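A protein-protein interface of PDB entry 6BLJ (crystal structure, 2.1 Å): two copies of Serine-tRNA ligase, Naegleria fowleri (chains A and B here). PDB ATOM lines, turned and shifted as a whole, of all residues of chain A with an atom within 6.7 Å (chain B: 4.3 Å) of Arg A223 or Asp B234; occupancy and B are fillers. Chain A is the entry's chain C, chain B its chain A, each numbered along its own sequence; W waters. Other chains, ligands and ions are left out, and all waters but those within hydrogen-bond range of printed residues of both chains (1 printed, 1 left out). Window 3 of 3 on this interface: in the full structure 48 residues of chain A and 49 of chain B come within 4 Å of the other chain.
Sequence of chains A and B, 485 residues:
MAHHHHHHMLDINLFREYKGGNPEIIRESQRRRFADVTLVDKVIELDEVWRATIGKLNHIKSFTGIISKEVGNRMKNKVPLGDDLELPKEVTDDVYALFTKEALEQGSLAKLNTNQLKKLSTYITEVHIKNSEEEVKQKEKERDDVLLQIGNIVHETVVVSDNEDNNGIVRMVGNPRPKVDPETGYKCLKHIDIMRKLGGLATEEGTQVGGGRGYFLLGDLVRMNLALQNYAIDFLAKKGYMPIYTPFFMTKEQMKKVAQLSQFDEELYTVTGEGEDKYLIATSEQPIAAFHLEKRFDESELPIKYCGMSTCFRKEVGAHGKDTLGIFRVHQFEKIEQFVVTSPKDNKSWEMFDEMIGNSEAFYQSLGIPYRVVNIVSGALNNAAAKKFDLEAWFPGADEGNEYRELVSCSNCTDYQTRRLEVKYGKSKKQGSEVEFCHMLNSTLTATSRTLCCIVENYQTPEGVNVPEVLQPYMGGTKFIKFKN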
ATOM      1  N   LEU A 218      19.856  21.290   8.750  1.00  0.00           N
ATOM      2  CA  LEU A 218      18.917  20.645   7.835  1.00  0.00           C
ATOM      3  C   LEU A 218      19.608  19.556   7.016  1.00  0.00           C
ATOM      4  O   LEU A 218      20.795  19.652   6.692  1.00  0.00           O
ATOM      5  CB  LEU A 218      18.281  21.643   6.858  1.00  0.00           C
ATOM      6  CG  LEU A 218      17.384  22.758   7.402  1.00  0.00           C
ATOM      7  CD1 LEU A 218      18.214  23.932   7.863  1.00  0.00           C
ATOM      8  CD2 LEU A 218      16.435  23.195   6.310  1.00  0.00           C
ATOM      9  N   GLY A 219      18.838  18.525   6.667  1.00  0.00           N
ATOM     10  CA  GLY A 219      19.276  17.565   5.661  1.00  0.00           C
ATOM     11  C   GLY A 219      20.387  16.646   6.140  1.00  0.00           C
ATOM     12  O   GLY A 219      20.398  16.181   7.289  1.00  0.00           O
ATOM     13  N   ASP A 220      21.337  16.372   5.233  1.00  0.00           N
ATOM     14  CA  ASP A 220      22.358  15.366   5.506  1.00  0.00           C
ATOM     15  C   ASP A 220      23.243  15.766   6.678  1.00  0.00           C
ATOM     16  O   ASP A 220      23.780  14.895   7.371  1.00  0.00           O
ATOM     17  CB  ASP A 220      23.224  15.133   4.260  1.00  0.00           C
ATOM     18  CG  ASP A 220      22.484  14.402   3.150  1.00  0.00           C
ATOM     19  OD1 ASP A 220      21.470  13.724   3.428  1.00  0.00           O
ATOM     20  OD2 ASP A 220      22.935  14.495   1.991  1.00  0.00           O
ATOM     21  N   LEU A 221      23.418  17.072   6.910  1.00  0.00           N
ATOM     22  CA  LEU A 221      24.215  17.524   8.046  1.00  0.00           C
ATOM     23  C   LEU A 221      23.588  17.083   9.360  1.00  0.00           C
ATOM     24  O   LEU A 221      24.305  16.765  10.321  1.00  0.00           O
ATOM     25  CB  LEU A 221      24.376  19.048   8.011  1.00  0.00           C
ATOM     26  CG  LEU A 221      25.361  19.717   7.032  1.00  0.00           C
ATOM     27  CD1 LEU A 221      25.367  21.256   7.239  1.00  0.00           C
ATOM     28  CD2 LEU A 221      26.792  19.139   7.126  1.00  0.00           C
ATOM     29  N   VAL A 222      22.249  17.074   9.431  1.00  0.00           N
ATOM     30  CA  VAL A 222      21.574  16.539  10.618  1.00  0.00           C
ATOM     31  C   VAL A 222      21.922  15.068  10.790  1.00  0.00           C
ATOM     32  O   VAL A 222      22.254  14.607  11.892  1.00  0.00           O
ATOM     33  CB  VAL A 222      20.047  16.737  10.526  1.00  0.00           C
ATOM     34  CG1 VAL A 222      19.340  16.084  11.749  1.00  0.00           C
ATOM     35  CG2 VAL A 222      19.669  18.208  10.414  1.00  0.00           C
ATOM     36  N   ARG A 223      21.812  14.301   9.704  1.00  0.00           N
ATOM     37  CA  ARG A 223      22.116  12.877   9.777  1.00  0.00           C
ATOM     38  C   ARG A 223      23.581  12.644  10.139  1.00  0.00           C
ATOM     39  O   ARG A 223      23.904  11.695  10.864  1.00  0.00           O
ATOM     40  CB  ARG A 223      21.745  12.198   8.457  1.00  0.00           C
ATOM     41  CG  ARG A 223      20.248  12.272   8.168  1.00  0.00           C
ATOM     42  CD  ARG A 223      19.840  11.310   7.061  1.00  0.00           C
ATOM     43  NE  ARG A 223      20.524  11.610   5.809  1.00  0.00           N
ATOM     44  CZ  ARG A 223      21.389  10.793   5.219  1.00  0.00           C
ATOM     45  NH1 ARG A 223      21.697   9.637   5.790  1.00  0.00           N
ATOM     46  NH2 ARG A 223      21.962  11.139   4.070  1.00  0.00           N
ATOM     47  N   MET A 224      24.484  13.511   9.667  1.00  0.00           N
ATOM     48  CA  MET A 224      25.884  13.372  10.055  1.00  0.00           C
ATOM     49  C   MET A 224      26.079  13.729  11.522  1.00  0.00           C
ATOM     50  O   MET A 224      26.910  13.119  12.211  1.00  0.00           O
ATOM     51  CB  MET A 224      26.791  14.250   9.192  1.00  0.00           C
ATOM     52  CG  MET A 224      28.276  13.904   9.359  1.00  0.00           C
ATOM     53  SD  MET A 224      29.364  14.818   8.242  1.00  0.00           S
ATOM     54  CE  MET A 224      29.002  14.015   6.698  1.00  0.00           C
ATOM     55  N   ASN A 225      25.319  14.710  12.016  1.00  0.00           N
ATOM     56  CA  ASN A 225      25.370  15.055  13.435  1.00  0.00           C
ATOM     57  C   ASN A 225      25.046  13.835  14.285  1.00  0.00           C
ATOM     58  O   ASN A 225      25.796  13.479  15.204  1.00  0.00           O
ATOM     59  CB  ASN A 225      24.378  16.194  13.729  1.00  0.00           C
ATOM     60  CG  ASN A 225      24.803  17.061  14.916  1.00  0.00           C
ATOM     61  OD1 ASN A 225      25.983  17.162  15.218  1.00  0.00           O
ATOM     62  ND2 ASN A 225      23.843  17.712  15.562  1.00  0.00           N
ATOM     63  N   LEU A 226      23.955  13.144  13.944  1.00  0.00           N
ATOM     64  CA  LEU A 226      23.582  11.926  14.650  1.00  0.00           C
ATOM     65  C   LEU A 226      24.633  10.841  14.480  1.00  0.00           C
ATOM     66  O   LEU A 226      24.960  10.128  15.439  1.00  0.00           O
ATOM     67  CB  LEU A 226      22.238  11.399  14.144  1.00  0.00           C
ATOM     68  CG  LEU A 226      21.076  11.477  15.114  1.00  0.00           C
ATOM     69  CD1 LEU A 226      19.931  10.697  14.552  1.00  0.00           C
ATOM     70  CD2 LEU A 226      21.499  10.917  16.459  1.00  0.00           C
ATOM     71  N   ALA A 227      25.157  10.691  13.258  1.00  0.00           N
ATOM     72  CA  ALA A 227      26.165   9.670  13.010  1.00  0.00           C
ATOM     73  C   ALA A 227      27.360   9.850  13.936  1.00  0.00           C
ATOM     74  O   ALA A 227      27.855   8.871  14.510  1.00  0.00           O
ATOM     75  CB  ALA A 227      26.602   9.707  11.544  1.00  0.00           C
ATOM     76  N   LEU A 228      27.807  11.100  14.132  1.00  0.00           N
ATOM     77  CA  LEU A 228      28.927  11.360  15.040  1.00  0.00           C
ATOM     78  C   LEU A 228      28.607  10.920  16.457  1.00  0.00           C
ATOM     79  O   LEU A 228      29.447  10.303  17.128  1.00  0.00           O
ATOM     80  CB  LEU A 228      29.286  12.849  15.044  1.00  0.00           C
ATOM     81  CG  LEU A 228      30.350  13.418  14.108  1.00  0.00           C
ATOM     82  CD1 LEU A 228      30.354  14.920  14.249  1.00  0.00           C
ATOM     83  CD2 LEU A 228      31.727  12.868  14.476  1.00  0.00           C
ATOM     84  N   TYR A 474      27.021   4.763   9.454  1.00  0.00           N
ATOM     85  CA  TYR A 474      26.133   5.440  10.384  1.00  0.00           C
ATOM     86  C   TYR A 474      25.189   6.417   9.700  1.00  0.00           C
ATOM     87  O   TYR A 474      24.316   6.980  10.372  1.00  0.00           O
ATOM     88  CB  TYR A 474      26.952   6.169  11.451  1.00  0.00           C
ATOM     89  CG  TYR A 474      27.637   5.239  12.421  1.00  0.00           C
ATOM     90  CD1 TYR A 474      26.976   4.785  13.550  1.00  0.00           C
ATOM     91  CD2 TYR A 474      28.937   4.797  12.196  1.00  0.00           C
ATOM     92  CE1 TYR A 474      27.595   3.922  14.449  1.00  0.00           C
ATOM     93  CE2 TYR A 474      29.569   3.938  13.082  1.00  0.00           C
ATOM     94  CZ  TYR A 474      28.890   3.509  14.214  1.00  0.00           C
ATOM     95  OH  TYR A 474      29.502   2.658  15.105  1.00  0.00           O
ATOM     96  N   MET A 475      25.317   6.602   8.387  1.00  0.00           N
ATOM     97  CA  MET A 475      24.452   7.497   7.625  1.00  0.00           C
ATOM     98  C   MET A 475      23.745   6.775   6.487  1.00  0.00           C
ATOM     99  O   MET A 475      23.479   7.372   5.444  1.00  0.00           O
ATOM    100  CB  MET A 475      25.246   8.670   7.059  1.00  0.00           C
ATOM    101  CG  MET A 475      25.483   9.776   8.037  1.00  0.00           C
ATOM    102  SD  MET A 475      26.393  11.051   7.202  1.00  0.00           S
ATOM    103  CE  MET A 475      25.141  11.774   6.160  1.00  0.00           C
ATOM    104  N   GLY A 476      23.431   5.496   6.678  1.00  0.00           N
ATOM    105  CA  GLY A 476      22.758   4.733   5.643  1.00  0.00           C
ATOM    106  C   GLY A 476      23.551   4.603   4.367  1.00  0.00           C
ATOM    107  O   GLY A 476      22.963   4.447   3.291  1.00  0.00           O
ATOM    108  N   GLY A 477      24.880   4.670   4.455  1.00  0.00           N
ATOM    109  CA  GLY A 477      25.751   4.461   3.322  1.00  0.00           C
ATOM    110  C   GLY A 477      26.078   5.687   2.490  1.00  0.00           C
ATOM    111  O   GLY A 477      26.824   5.560   1.510  1.00  0.00           O
ATOM    112  N   THR A 478      25.564   6.862   2.848  1.00  0.00           N
ATOM    113  CA  THR A 478      25.842   8.070   2.078  1.00  0.00           C
ATOM    114  C   THR A 478      27.342   8.342   1.999  1.00  0.00           C
ATOM    115  O   THR A 478      28.035   8.395   3.021  1.00  0.00           O
ATOM    116  CB  THR A 478      25.132   9.262   2.708  1.00  0.00           C
ATOM    117  OG1 THR A 478      23.730   8.997   2.779  1.00  0.00           O
ATOM    118  CG2 THR A 478      25.377  10.530   1.887  1.00  0.00           C
ATOM    119  N   ILE A 481      27.909  14.482  -0.114  1.00  0.00           N
ATOM    120  CA  ILE A 481      26.834  15.465  -0.011  1.00  0.00           C
ATOM    121  C   ILE A 481      27.112  16.537  -1.048  1.00  0.00           C
ATOM    122  O   ILE A 481      28.116  17.247  -0.947  1.00  0.00           O
ATOM    123  CB  ILE A 481      26.751  16.076   1.397  1.00  0.00           C
ATOM    124  CG1 ILE A 481      26.849  15.000   2.480  1.00  0.00           C
ATOM    125  CG2 ILE A 481      25.458  16.892   1.559  1.00  0.00           C
ATOM    126  CD1 ILE A 481      26.985  15.605   3.900  1.00  0.00           C
ATOM    127  N   ASN B 230      17.854   7.643  15.342  1.00  0.00           N
ATOM    128  CA  ASN B 230      18.518   7.437  14.058  1.00  0.00           C
ATOM    129  C   ASN B 230      17.584   6.762  13.054  1.00  0.00           C
ATOM    130  O   ASN B 230      17.529   7.145  11.875  1.00  0.00           O
ATOM    131  CB  ASN B 230      19.771   6.593  14.288  1.00  0.00           C
ATOM    132  CG  ASN B 230      20.823   6.773  13.208  1.00  0.00           C
ATOM    133  OD1 ASN B 230      22.018   6.758  13.486  1.00  0.00           O
ATOM    134  ND2 ASN B 230      20.381   6.932  11.966  1.00  0.00           N
ATOM    135  N   TYR B 231      16.871   5.729  13.501  1.00  0.00           N
ATOM    136  CA  TYR B 231      15.933   5.025  12.636  1.00  0.00           C
ATOM    137  C   TYR B 231      14.773   5.933  12.238  1.00  0.00           C
ATOM    138  O   TYR B 231      14.391   5.984  11.064  1.00  0.00           O
ATOM    139  CB  TYR B 231      15.428   3.761  13.346  1.00  0.00           C
ATOM    140  CG  TYR B 231      14.265   3.068  12.654  1.00  0.00           C
ATOM    141  CD1 TYR B 231      14.330   2.761  11.303  1.00  0.00           C
ATOM    142  CD2 TYR B 231      13.111   2.719  13.354  1.00  0.00           C
ATOM    143  CE1 TYR B 231      13.271   2.133  10.651  1.00  0.00           C
ATOM    144  CE2 TYR B 231      12.039   2.080  12.710  1.00  0.00           C
ATOM    145  CZ  TYR B 231      12.137   1.793  11.353  1.00  0.00           C
ATOM    146  OH  TYR B 231      11.103   1.175  10.688  1.00  0.00           O
ATOM    147  N   ALA B 232      14.221   6.674  13.199  1.00  0.00           N
ATOM    148  CA  ALA B 232      13.098   7.561  12.903  1.00  0.00           C
ATOM    149  C   ALA B 232      13.460   8.572  11.827  1.00  0.00           C
ATOM    150  O   ALA B 232      12.685   8.809  10.891  1.00  0.00           O
ATOM    151  CB  ALA B 232      12.653   8.284  14.175  1.00  0.00           C
ATOM    152  N   ILE B 233      14.642   9.175  11.939  1.00  0.00           N
ATOM    153  CA  ILE B 233      15.061  10.166  10.948  1.00  0.00           C
ATOM    154  C   ILE B 233      15.276   9.510   9.585  1.00  0.00           C
ATOM    155  O   ILE B 233      14.867  10.054   8.549  1.00  0.00           O
ATOM    156  CB  ILE B 233      16.311  10.907  11.464  1.00  0.00           C
ATOM    157  CG1 ILE B 233      15.885  11.854  12.596  1.00  0.00           C
ATOM    158  CG2 ILE B 233      17.005  11.675  10.359  1.00  0.00           C
ATOM    159  CD1 ILE B 233      16.972  12.197  13.537  1.00  0.00           C
ATOM    160  N   ASP B 234      15.912   8.335   9.554  1.00  0.00           N
ATOM    161  CA  ASP B 234      16.053   7.614   8.285  1.00  0.00           C
ATOM    162  C   ASP B 234      14.687   7.279   7.699  1.00  0.00           C
ATOM    163  O   ASP B 234      14.441   7.474   6.504  1.00  0.00           O
ATOM    164  CB  ASP B 234      16.864   6.338   8.483  1.00  0.00           C
ATOM    165  CG  ASP B 234      18.330   6.606   8.629  1.00  0.00           C
ATOM    166  OD1 ASP B 234      18.733   7.770   8.401  1.00  0.00           O
ATOM    167  OD2 ASP B 234      19.076   5.650   8.939  1.00  0.00           O
ATOM    168  N   PHE B 235      13.788   6.776   8.549  1.00  0.00           N
ATOM    169  CA  PHE B 235      12.434   6.409   8.142  1.00  0.00           C
ATOM    170  C   PHE B 235      11.724   7.578   7.459  1.00  0.00           C
ATOM    171  O   PHE B 235      11.188   7.439   6.354  1.00  0.00           O
ATOM    172  CB  PHE B 235      11.692   5.949   9.401  1.00  0.00           C
ATOM    173  CG  PHE B 235      10.280   5.466   9.181  1.00  0.00           C
ATOM    174  CD1 PHE B 235      10.028   4.151   8.834  1.00  0.00           C
ATOM    175  CD2 PHE B 235       9.207   6.310   9.405  1.00  0.00           C
ATOM    176  CE1 PHE B 235       8.731   3.698   8.681  1.00  0.00           C
ATOM    177  CE2 PHE B 235       7.909   5.861   9.243  1.00  0.00           C
ATOM    178  CZ  PHE B 235       7.677   4.550   8.889  1.00  0.00           C
ATOM    179  N   LEU B 236      11.735   8.754   8.089  1.00  0.00           N
ATOM    180  CA  LEU B 236      11.039   9.889   7.491  1.00  0.00           C
ATOM    181  C   LEU B 236      11.804  10.503   6.321  1.00  0.00           C
ATOM    182  O   LEU B 236      11.176  10.979   5.365  1.00  0.00           O
ATOM    183  CB  LEU B 236      10.758  10.957   8.554  1.00  0.00           C
ATOM    184  CG  LEU B 236       9.595  10.640   9.501  1.00  0.00           C
ATOM    185  CD1 LEU B 236       9.410  11.758  10.540  1.00  0.00           C
ATOM    186  CD2 LEU B 236       8.299  10.406   8.708  1.00  0.00           C
ATOM    187  N   ALA B 237      13.143  10.516   6.373  1.00  0.00           N
ATOM    188  CA  ALA B 237      13.916  11.064   5.259  1.00  0.00           C
ATOM    189  C   ALA B 237      13.629  10.300   3.977  1.00  0.00           C
ATOM    190  O   ALA B 237      13.537  10.894   2.895  1.00  0.00           O
ATOM    191  CB  ALA B 237      15.417  11.030   5.563  1.00  0.00           C
ATOM    192  N   LYS B 238      13.509   8.981   4.079  1.00  0.00           N
ATOM    193  CA  LYS B 238      13.176   8.170   2.922  1.00  0.00           C
ATOM    194  C   LYS B 238      11.770   8.448   2.406  1.00  0.00           C
ATOM    195  O   LYS B 238      11.499   8.195   1.229  1.00  0.00           O
ATOM    196  CB  LYS B 238      13.387   6.696   3.260  1.00  0.00           C
ATOM    197  CG  LYS B 238      14.878   6.378   3.339  1.00  0.00           C
ATOM    198  CD  LYS B 238      15.218   4.976   3.815  1.00  0.00           C
ATOM    199  CE  LYS B 238      16.738   4.827   3.860  1.00  0.00           C
ATOM    200  NZ  LYS B 238      17.211   3.552   4.455  1.00  0.00           N
ATOM    201  N   TYR B 474      20.832  -0.649  14.133  1.00  0.00           N
ATOM    202  CA  TYR B 474      21.139   0.666  14.674  1.00  0.00           C
ATOM    203  C   TYR B 474      21.816   0.599  16.035  1.00  0.00           C
ATOM    204  O   TYR B 474      22.175   1.645  16.587  1.00  0.00           O
ATOM    205  CB  TYR B 474      19.857   1.494  14.774  1.00  0.00           C
ATOM    206  CG  TYR B 474      19.269   1.896  13.437  1.00  0.00           C
ATOM    207  CD1 TYR B 474      19.681   3.055  12.806  1.00  0.00           C
ATOM    208  CD2 TYR B 474      18.300   1.115  12.813  1.00  0.00           C
ATOM    209  CE1 TYR B 474      19.146   3.433  11.583  1.00  0.00           C
ATOM    210  CE2 TYR B 474      17.756   1.490  11.593  1.00  0.00           C
ATOM    211  CZ  TYR B 474      18.184   2.657  10.989  1.00  0.00           C
ATOM    212  OH  TYR B 474      17.669   3.055   9.777  1.00  0.00           O
HETATM  213  O   HOH W   1      22.511   9.206  10.900  1.00  0.00           O
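Among the printed residues, pairs that only touch across the chains: Arg A223 with Ile B233 (3.96 Å), Arg A223 with Asp B234 (3.9 Å), Leu A226 with Asn B230 (3.6 Å), Leu A226 with Ile B233 (3.5 Å) and Tyr A474 with Asn B230 (3.9 Å).
Val A222 touches none of the printed residues of chain B. Of the printed residues of chain B, Leu A226 touches Asn B230 and Ile B233. Printed residues of chain A within 4 Å of Asn B230: Leu A226 and Tyr A474. Printed residues of chain A within 4 Å of Ile B233: Arg A223 (3.96 Å) and Leu A226 (3.5 Å). Of chain A, only Arg A223 comes within 4 Å of Asp B234. The nearest printed residue of chain B that does not touch Arg A223 is Ala B237 (4.7 Å). The nearest printed residue of chain B that does not touch Tyr A474 is Asp B234 (5.6 Å).
Water W1 lies within hydrogen-bond range of O of Arg A223 (2.9 Å), O of Tyr A474 (2.9 Å) and ND2 of Asn B230 (3.3 Å).
Among the printed residues, 5 pairs touch across the chains.
The side-chain carboxylate of Asp B234 is in hydrogen-bond range of the side-chain hydroxyl of Tyr B474. The guanidinium group (NH2) of Arg A223 lies within salt-bridge range of the side-chain carboxylate (OD1) of Asp A220 (2.7 Å). The backbone carbonyl oxygen of Met A475 lies within hydrogen-bond range of the guanidinium group of Arg A223. The guanidinium group of Arg A223 sits at hydrogen-bond distance from the side-chain hydroxyl of Thr A478.
Position printed for both chains: 474. Of the 5 pairs that touch across the chains among the printed residues, none has its exchanged pair printed and touching as well.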
